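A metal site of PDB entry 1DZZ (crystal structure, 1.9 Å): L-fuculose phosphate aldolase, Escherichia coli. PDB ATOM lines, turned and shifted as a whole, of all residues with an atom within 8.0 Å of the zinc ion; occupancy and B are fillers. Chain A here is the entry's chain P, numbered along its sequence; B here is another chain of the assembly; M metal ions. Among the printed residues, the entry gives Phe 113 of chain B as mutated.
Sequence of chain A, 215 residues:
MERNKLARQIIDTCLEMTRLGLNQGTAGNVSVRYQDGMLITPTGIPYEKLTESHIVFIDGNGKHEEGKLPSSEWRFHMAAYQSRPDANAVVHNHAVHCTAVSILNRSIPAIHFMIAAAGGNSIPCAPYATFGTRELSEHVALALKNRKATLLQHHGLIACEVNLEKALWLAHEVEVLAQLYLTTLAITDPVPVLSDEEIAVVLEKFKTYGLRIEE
The zinc ion is bound by NE2 of His 92 (2.2 Å), NE2 of His 94 (2.2 Å), NE2 of His 155 (2.2 Å), OE2 of Glu 73 (2.5 Å) and OE1 of Glu 73 (2.5 Å).
The zinc ion has five donor atoms within binding distance.
Within 4 Å of the zinc ion: Glu 73, His 92, His 94 and His 155.
OG of Ser 71 sits at hydrogen-bond distance from N of Glu 73, at 3.0 Å.
The side-chain carboxylate (OE2) of Glu 73 sits close to the side-chain amide nitrogen (ND2) of Asn 29.
The backbone carbonyl oxygen of His 155 is in hydrogen-bond range of a ring nitrogen (NE2) of His 112 of chain B, at 2.8 Å.
The backbone carbonyl oxygen (O) of Asn 29 lies within hydrogen-bond range of the backbone NH (N) of His 92.
ND1 of His 92 lies within hydrogen-bond range of O of Leu 157, 2.7 Å away.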
ATOM      1  N   THR A  26     -27.658 -27.724 -16.075  1.00  0.00           N
ATOM      2  CA  THR A  26     -26.284 -28.041 -15.685  1.00  0.00           C
ATOM      3  C   THR A  26     -25.281 -27.785 -16.799  1.00  0.00           C
ATOM      4  O   THR A  26     -24.175 -28.346 -16.791  1.00  0.00           O
ATOM      5  CB  THR A  26     -26.212 -29.522 -15.249  1.00  0.00           C
ATOM      6  OG1 THR A  26     -26.725 -30.360 -16.306  1.00  0.00           O
ATOM      7  CG2 THR A  26     -27.019 -29.722 -13.970  1.00  0.00           C
ATOM      8  N   ALA A  27     -25.649 -26.928 -17.751  1.00  0.00           N
ATOM      9  CA  ALA A  27     -24.837 -26.693 -18.925  1.00  0.00           C
ATOM     10  C   ALA A  27     -23.488 -26.032 -18.721  1.00  0.00           C
ATOM     11  O   ALA A  27     -22.473 -26.568 -19.196  1.00  0.00           O
ATOM     12  CB  ALA A  27     -25.711 -25.939 -19.913  1.00  0.00           C
ATOM     13  N   GLY A  28     -23.344 -24.877 -18.089  1.00  0.00           N
ATOM     14  CA  GLY A  28     -22.054 -24.227 -18.022  1.00  0.00           C
ATOM     15  C   GLY A  28     -20.995 -24.803 -17.094  1.00  0.00           C
ATOM     16  O   GLY A  28     -21.213 -25.661 -16.246  1.00  0.00           O
ATOM     17  N   ASN A  29     -19.754 -24.364 -17.332  1.00  0.00           N
ATOM     18  CA  ASN A  29     -18.613 -24.745 -16.491  1.00  0.00           C
ATOM     19  C   ASN A  29     -17.723 -23.503 -16.477  1.00  0.00           C
ATOM     20  O   ASN A  29     -17.655 -22.743 -17.448  1.00  0.00           O
ATOM     21  CB  ASN A  29     -17.949 -26.051 -16.869  1.00  0.00           C
ATOM     22  CG  ASN A  29     -18.063 -26.447 -18.308  1.00  0.00           C
ATOM     23  OD1 ASN A  29     -17.297 -25.943 -19.128  1.00  0.00           O
ATOM     24  ND2 ASN A  29     -18.996 -27.330 -18.686  1.00  0.00           N
ATOM     25  N   SER A  71     -15.526 -31.061 -14.161  1.00  0.00           N
ATOM     26  CA  SER A  71     -16.473 -30.923 -15.264  1.00  0.00           C
ATOM     27  C   SER A  71     -16.059 -31.893 -16.367  1.00  0.00           C
ATOM     28  O   SER A  71     -14.841 -32.013 -16.608  1.00  0.00           O
ATOM     29  CB  SER A  71     -16.363 -29.487 -15.814  1.00  0.00           C
ATOM     30  OG  SER A  71     -16.901 -29.480 -17.121  1.00  0.00           O
ATOM     31  N   SER A  72     -17.017 -32.409 -17.139  1.00  0.00           N
ATOM     32  CA  SER A  72     -16.637 -33.334 -18.215  1.00  0.00           C
ATOM     33  C   SER A  72     -15.905 -32.627 -19.340  1.00  0.00           C
ATOM     34  O   SER A  72     -15.230 -33.261 -20.162  1.00  0.00           O
ATOM     35  CB  SER A  72     -17.881 -34.043 -18.771  1.00  0.00           C
ATOM     36  OG  SER A  72     -18.800 -33.057 -19.261  1.00  0.00           O
ATOM     37  N   GLU A  73     -15.964 -31.301 -19.375  1.00  0.00           N
ATOM     38  CA  GLU A  73     -15.318 -30.473 -20.369  1.00  0.00           C
ATOM     39  C   GLU A  73     -14.068 -29.757 -19.906  1.00  0.00           C
ATOM     40  O   GLU A  73     -13.642 -28.798 -20.553  1.00  0.00           O
ATOM     41  CB  GLU A  73     -16.377 -29.428 -20.800  1.00  0.00           C
ATOM     42  CG  GLU A  73     -17.700 -30.129 -21.111  1.00  0.00           C
ATOM     43  CD  GLU A  73     -18.650 -29.277 -21.926  1.00  0.00           C
ATOM     44  OE1 GLU A  73     -18.582 -29.342 -23.172  1.00  0.00           O
ATOM     45  OE2 GLU A  73     -19.448 -28.561 -21.311  1.00  0.00           O
ATOM     46  N   PHE A  76     -10.926 -28.580 -22.545  1.00  0.00           N
ATOM     47  CA  PHE A  76     -10.787 -27.357 -23.363  1.00  0.00           C
ATOM     48  C   PHE A  76     -10.563 -26.148 -22.449  1.00  0.00           C
ATOM     49  O   PHE A  76     -10.109 -25.130 -22.984  1.00  0.00           O
ATOM     50  CB  PHE A  76     -11.839 -27.202 -24.413  1.00  0.00           C
ATOM     51  CG  PHE A  76     -13.284 -27.057 -24.043  1.00  0.00           C
ATOM     52  CD1 PHE A  76     -13.687 -26.177 -23.042  1.00  0.00           C
ATOM     53  CD2 PHE A  76     -14.257 -27.770 -24.732  1.00  0.00           C
ATOM     54  CE1 PHE A  76     -15.031 -26.035 -22.717  1.00  0.00           C
ATOM     55  CE2 PHE A  76     -15.601 -27.606 -24.409  1.00  0.00           C
ATOM     56  CZ  PHE A  76     -15.985 -26.755 -23.384  1.00  0.00           C
ATOM     57  N   HIS A  77     -10.802 -26.212 -21.150  1.00  0.00           N
ATOM     58  CA  HIS A  77     -10.407 -25.109 -20.271  1.00  0.00           C
ATOM     59  C   HIS A  77      -8.879 -25.105 -20.249  1.00  0.00           C
ATOM     60  O   HIS A  77      -8.256 -24.054 -20.402  1.00  0.00           O
ATOM     61  CB  HIS A  77     -10.893 -25.296 -18.826  1.00  0.00           C
ATOM     62  CG  HIS A  77     -12.365 -25.041 -18.740  1.00  0.00           C
ATOM     63  ND1 HIS A  77     -12.870 -23.876 -18.202  1.00  0.00           N
ATOM     64  CD2 HIS A  77     -13.413 -25.780 -19.170  1.00  0.00           C
ATOM     65  CE1 HIS A  77     -14.186 -23.910 -18.280  1.00  0.00           C
ATOM     66  NE2 HIS A  77     -14.538 -25.051 -18.874  1.00  0.00           N
ATOM     67  N   HIS A  92     -17.708 -21.126 -19.968  1.00  0.00           N
ATOM     68  CA  HIS A  92     -18.309 -21.898 -21.058  1.00  0.00           C
ATOM     69  C   HIS A  92     -19.801 -22.059 -20.761  1.00  0.00           C
ATOM     70  O   HIS A  92     -20.200 -22.373 -19.647  1.00  0.00           O
ATOM     71  CB  HIS A  92     -17.622 -23.260 -21.178  1.00  0.00           C
ATOM     72  CG  HIS A  92     -18.346 -24.196 -22.113  1.00  0.00           C
ATOM     73  ND1 HIS A  92     -18.551 -23.923 -23.437  1.00  0.00           N
ATOM     74  CD2 HIS A  92     -18.932 -25.387 -21.844  1.00  0.00           C
ATOM     75  CE1 HIS A  92     -19.203 -24.924 -23.994  1.00  0.00           C
ATOM     76  NE2 HIS A  92     -19.449 -25.787 -23.043  1.00  0.00           N
ATOM     77  N   ASN A  93     -20.662 -21.884 -21.762  1.00  0.00           N
ATOM     78  CA  ASN A  93     -22.083 -22.171 -21.533  1.00  0.00           C
ATOM     79  C   ASN A  93     -22.712 -22.553 -22.860  1.00  0.00           C
ATOM     80  O   ASN A  93     -22.029 -22.559 -23.888  1.00  0.00           O
ATOM     81  CB  ASN A  93     -22.772 -20.967 -20.920  1.00  0.00           C
ATOM     82  CG  ASN A  93     -22.681 -19.752 -21.815  1.00  0.00           C
ATOM     83  OD1 ASN A  93     -22.970 -19.805 -23.016  1.00  0.00           O
ATOM     84  ND2 ASN A  93     -22.301 -18.642 -21.178  1.00  0.00           N
ATOM     85  N   HIS A  94     -23.985 -22.867 -22.827  1.00  0.00           N
ATOM     86  CA  HIS A  94     -24.720 -23.253 -24.018  1.00  0.00           C
ATOM     87  C   HIS A  94     -25.835 -22.198 -24.195  1.00  0.00           C
ATOM     88  O   HIS A  94     -26.993 -22.538 -24.395  1.00  0.00           O
ATOM     89  CB  HIS A  94     -25.287 -24.670 -23.904  1.00  0.00           C
ATOM     90  CG  HIS A  94     -24.320 -25.789 -23.693  1.00  0.00           C
ATOM     91  ND1 HIS A  94     -24.763 -27.074 -23.469  1.00  0.00           N
ATOM     92  CD2 HIS A  94     -22.965 -25.897 -23.660  1.00  0.00           C
ATOM     93  CE1 HIS A  94     -23.745 -27.903 -23.274  1.00  0.00           C
ATOM     94  NE2 HIS A  94     -22.636 -27.195 -23.388  1.00  0.00           N
ATOM     95  N   PHE A 131     -17.707 -33.687 -27.359  1.00  0.00           N
ATOM     96  CA  PHE A 131     -17.312 -33.023 -26.115  1.00  0.00           C
ATOM     97  C   PHE A 131     -16.271 -33.853 -25.357  1.00  0.00           C
ATOM     98  O   PHE A 131     -16.247 -35.099 -25.451  1.00  0.00           O
ATOM     99  CB  PHE A 131     -18.521 -32.755 -25.206  1.00  0.00           C
ATOM    100  CG  PHE A 131     -19.155 -33.959 -24.571  1.00  0.00           C
ATOM    101  CD1 PHE A 131     -20.093 -34.713 -25.255  1.00  0.00           C
ATOM    102  CD2 PHE A 131     -18.799 -34.354 -23.299  1.00  0.00           C
ATOM    103  CE1 PHE A 131     -20.661 -35.836 -24.683  1.00  0.00           C
ATOM    104  CE2 PHE A 131     -19.370 -35.485 -22.716  1.00  0.00           C
ATOM    105  CZ  PHE A 131     -20.312 -36.225 -23.402  1.00  0.00           C
ATOM    106  N   GLY A 132     -15.395 -33.194 -24.608  1.00  0.00           N
ATOM    107  CA  GLY A 132     -14.363 -33.846 -23.840  1.00  0.00           C
ATOM    108  C   GLY A 132     -13.260 -34.526 -24.594  1.00  0.00           C
ATOM    109  O   GLY A 132     -12.516 -35.325 -23.998  1.00  0.00           O
ATOM    110  N   LEU A 136     -11.535 -31.733 -29.944  1.00  0.00           N
ATOM    111  CA  LEU A 136     -12.248 -30.500 -29.616  1.00  0.00           C
ATOM    112  C   LEU A 136     -11.291 -29.435 -29.070  1.00  0.00           C
ATOM    113  O   LEU A 136     -11.358 -28.266 -29.439  1.00  0.00           O
ATOM    114  CB  LEU A 136     -13.344 -30.765 -28.588  1.00  0.00           C
ATOM    115  CG  LEU A 136     -14.697 -30.075 -28.681  1.00  0.00           C
ATOM    116  CD1 LEU A 136     -15.306 -29.874 -27.297  1.00  0.00           C
ATOM    117  CD2 LEU A 136     -14.710 -28.819 -29.516  1.00  0.00           C
ATOM    118  N   LEU A 152     -18.680 -22.788 -30.724  1.00  0.00           N
ATOM    119  CA  LEU A 152     -18.341 -24.191 -30.914  1.00  0.00           C
ATOM    120  C   LEU A 152     -19.509 -24.783 -31.719  1.00  0.00           C
ATOM    121  O   LEU A 152     -20.618 -24.747 -31.180  1.00  0.00           O
ATOM    122  CB  LEU A 152     -18.267 -24.927 -29.570  1.00  0.00           C
ATOM    123  CG  LEU A 152     -17.028 -24.605 -28.716  1.00  0.00           C
ATOM    124  CD1 LEU A 152     -17.221 -23.312 -27.954  1.00  0.00           C
ATOM    125  CD2 LEU A 152     -16.772 -25.716 -27.718  1.00  0.00           C
ATOM    126  N   HIS A 154     -22.480 -26.722 -33.139  1.00  0.00           N
ATOM    127  CA  HIS A 154     -23.444 -27.610 -32.547  1.00  0.00           C
ATOM    128  C   HIS A 154     -23.268 -27.738 -31.037  1.00  0.00           C
ATOM    129  O   HIS A 154     -23.571 -28.810 -30.483  1.00  0.00           O
ATOM    130  CB  HIS A 154     -23.368 -29.052 -33.104  1.00  0.00           C
ATOM    131  CG  HIS A 154     -23.955 -29.118 -34.461  1.00  0.00           C
ATOM    132  ND1 HIS A 154     -25.291 -28.917 -34.728  1.00  0.00           N
ATOM    133  CD2 HIS A 154     -23.338 -29.320 -35.664  1.00  0.00           C
ATOM    134  CE1 HIS A 154     -25.469 -29.001 -36.051  1.00  0.00           C
ATOM    135  NE2 HIS A 154     -24.312 -29.250 -36.627  1.00  0.00           N
ATOM    136  N   HIS A 155     -22.865 -26.627 -30.392  1.00  0.00           N
ATOM    137  CA  HIS A 155     -22.538 -26.836 -28.970  1.00  0.00           C
ATOM    138  C   HIS A 155     -22.772 -25.620 -28.107  1.00  0.00           C
ATOM    139  O   HIS A 155     -23.623 -25.681 -27.215  1.00  0.00           O
ATOM    140  CB  HIS A 155     -21.068 -27.309 -28.989  1.00  0.00           C
ATOM    141  CG  HIS A 155     -20.546 -27.689 -27.646  1.00  0.00           C
ATOM    142  ND1 HIS A 155     -19.606 -28.666 -27.491  1.00  0.00           N
ATOM    143  CD2 HIS A 155     -20.824 -27.249 -26.396  1.00  0.00           C
ATOM    144  CE1 HIS A 155     -19.318 -28.826 -26.194  1.00  0.00           C
ATOM    145  NE2 HIS A 155     -20.061 -27.960 -25.519  1.00  0.00           N
ATOM    146  N   GLY A 156     -22.030 -24.539 -28.329  1.00  0.00           N
ATOM    147  CA  GLY A 156     -22.158 -23.377 -27.454  1.00  0.00           C
ATOM    148  C   GLY A 156     -21.025 -22.367 -27.605  1.00  0.00           C
ATOM    149  O   GLY A 156     -20.561 -22.062 -28.700  1.00  0.00           O
ATOM    150  N   LEU A 157     -20.553 -21.841 -26.489  1.00  0.00           N
ATOM    151  CA  LEU A 157     -19.619 -20.729 -26.422  1.00  0.00           C
ATOM    152  C   LEU A 157     -18.510 -20.884 -25.394  1.00  0.00           C
ATOM    153  O   LEU A 157     -18.764 -21.394 -24.314  1.00  0.00           O
ATOM    154  CB  LEU A 157     -20.477 -19.531 -25.992  1.00  0.00           C
ATOM    155  CG  LEU A 157     -20.036 -18.103 -25.699  1.00  0.00           C
ATOM    156  CD1 LEU A 157     -19.372 -17.997 -24.339  1.00  0.00           C
ATOM    157  CD2 LEU A 157     -19.158 -17.438 -26.734  1.00  0.00           C
ATOM    158  N   ILE A 158     -17.323 -20.356 -25.682  1.00  0.00           N
ATOM    159  CA  ILE A 158     -16.254 -20.266 -24.691  1.00  0.00           C
ATOM    160  C   ILE A 158     -15.750 -18.816 -24.726  1.00  0.00           C
ATOM    161  O   ILE A 158     -15.549 -18.256 -25.810  1.00  0.00           O
ATOM    162  CB  ILE A 158     -15.018 -21.147 -24.924  1.00  0.00           C
ATOM    163  CG1 ILE A 158     -15.388 -22.590 -25.219  1.00  0.00           C
ATOM    164  CG2 ILE A 158     -14.149 -21.084 -23.660  1.00  0.00           C
ATOM    165  CD1 ILE A 158     -14.329 -23.456 -25.848  1.00  0.00           C
ATOM    166  N   HIS B 112     -28.312 -30.525 -31.942  1.00  0.00           N
ATOM    167  CA  HIS B 112     -27.396 -30.314 -30.828  1.00  0.00           C
ATOM    168  C   HIS B 112     -27.176 -31.654 -30.134  1.00  0.00           C
ATOM    169  O   HIS B 112     -28.107 -32.497 -30.062  1.00  0.00           O
ATOM    170  CB  HIS B 112     -28.030 -29.336 -29.838  1.00  0.00           C
ATOM    171  CG  HIS B 112     -27.048 -28.830 -28.813  1.00  0.00           C
ATOM    172  ND1 HIS B 112     -26.638 -29.539 -27.708  1.00  0.00           N
ATOM    173  CD2 HIS B 112     -26.365 -27.660 -28.792  1.00  0.00           C
ATOM    174  CE1 HIS B 112     -25.752 -28.840 -27.035  1.00  0.00           C
ATOM    175  NE2 HIS B 112     -25.584 -27.684 -27.664  1.00  0.00           N
ATOM    176  N   PHE B 113     -25.985 -31.884 -29.574  1.00  0.00           N
ATOM    177  CA  PHE B 113     -25.733 -33.210 -28.984  1.00  0.00           C
ATOM    178  C   PHE B 113     -26.520 -33.503 -27.724  1.00  0.00           C
ATOM    179  O   PHE B 113     -26.710 -34.691 -27.403  1.00  0.00           O
ATOM    180  CB  PHE B 113     -24.244 -33.488 -28.775  1.00  0.00           C
ATOM    181  CG  PHE B 113     -23.672 -32.620 -27.684  1.00  0.00           C
ATOM    182  CD1 PHE B 113     -23.720 -33.011 -26.365  1.00  0.00           C
ATOM    183  CD2 PHE B 113     -23.053 -31.436 -28.035  1.00  0.00           C
ATOM    184  CE1 PHE B 113     -23.172 -32.213 -25.376  1.00  0.00           C
ATOM    185  CE2 PHE B 113     -22.492 -30.614 -27.069  1.00  0.00           C
ATOM    186  CZ  PHE B 113     -22.572 -31.021 -25.747  1.00  0.00           C
ATOM    187  N   MET B 114     -27.086 -32.515 -27.051  1.00  0.00           N
ATOM    188  CA  MET B 114     -27.907 -32.746 -25.888  1.00  0.00           C
ATOM    189  C   MET B 114     -29.210 -33.452 -26.229  1.00  0.00           C
ATOM    190  O   MET B 114     -29.836 -33.920 -25.279  1.00  0.00           O
ATOM    191  CB  MET B 114     -28.206 -31.482 -25.088  1.00  0.00           C
ATOM    192  CG  MET B 114     -26.967 -31.033 -24.300  1.00  0.00           C
ATOM    193  SD  MET B 114     -26.447 -32.235 -23.050  1.00  0.00           S
ATOM    194  CE  MET B 114     -27.949 -32.351 -22.082  1.00  0.00           C
HETATM  195 ZN    ZN M   1     -20.484 -27.679 -23.356  1.00  0.00          ZN
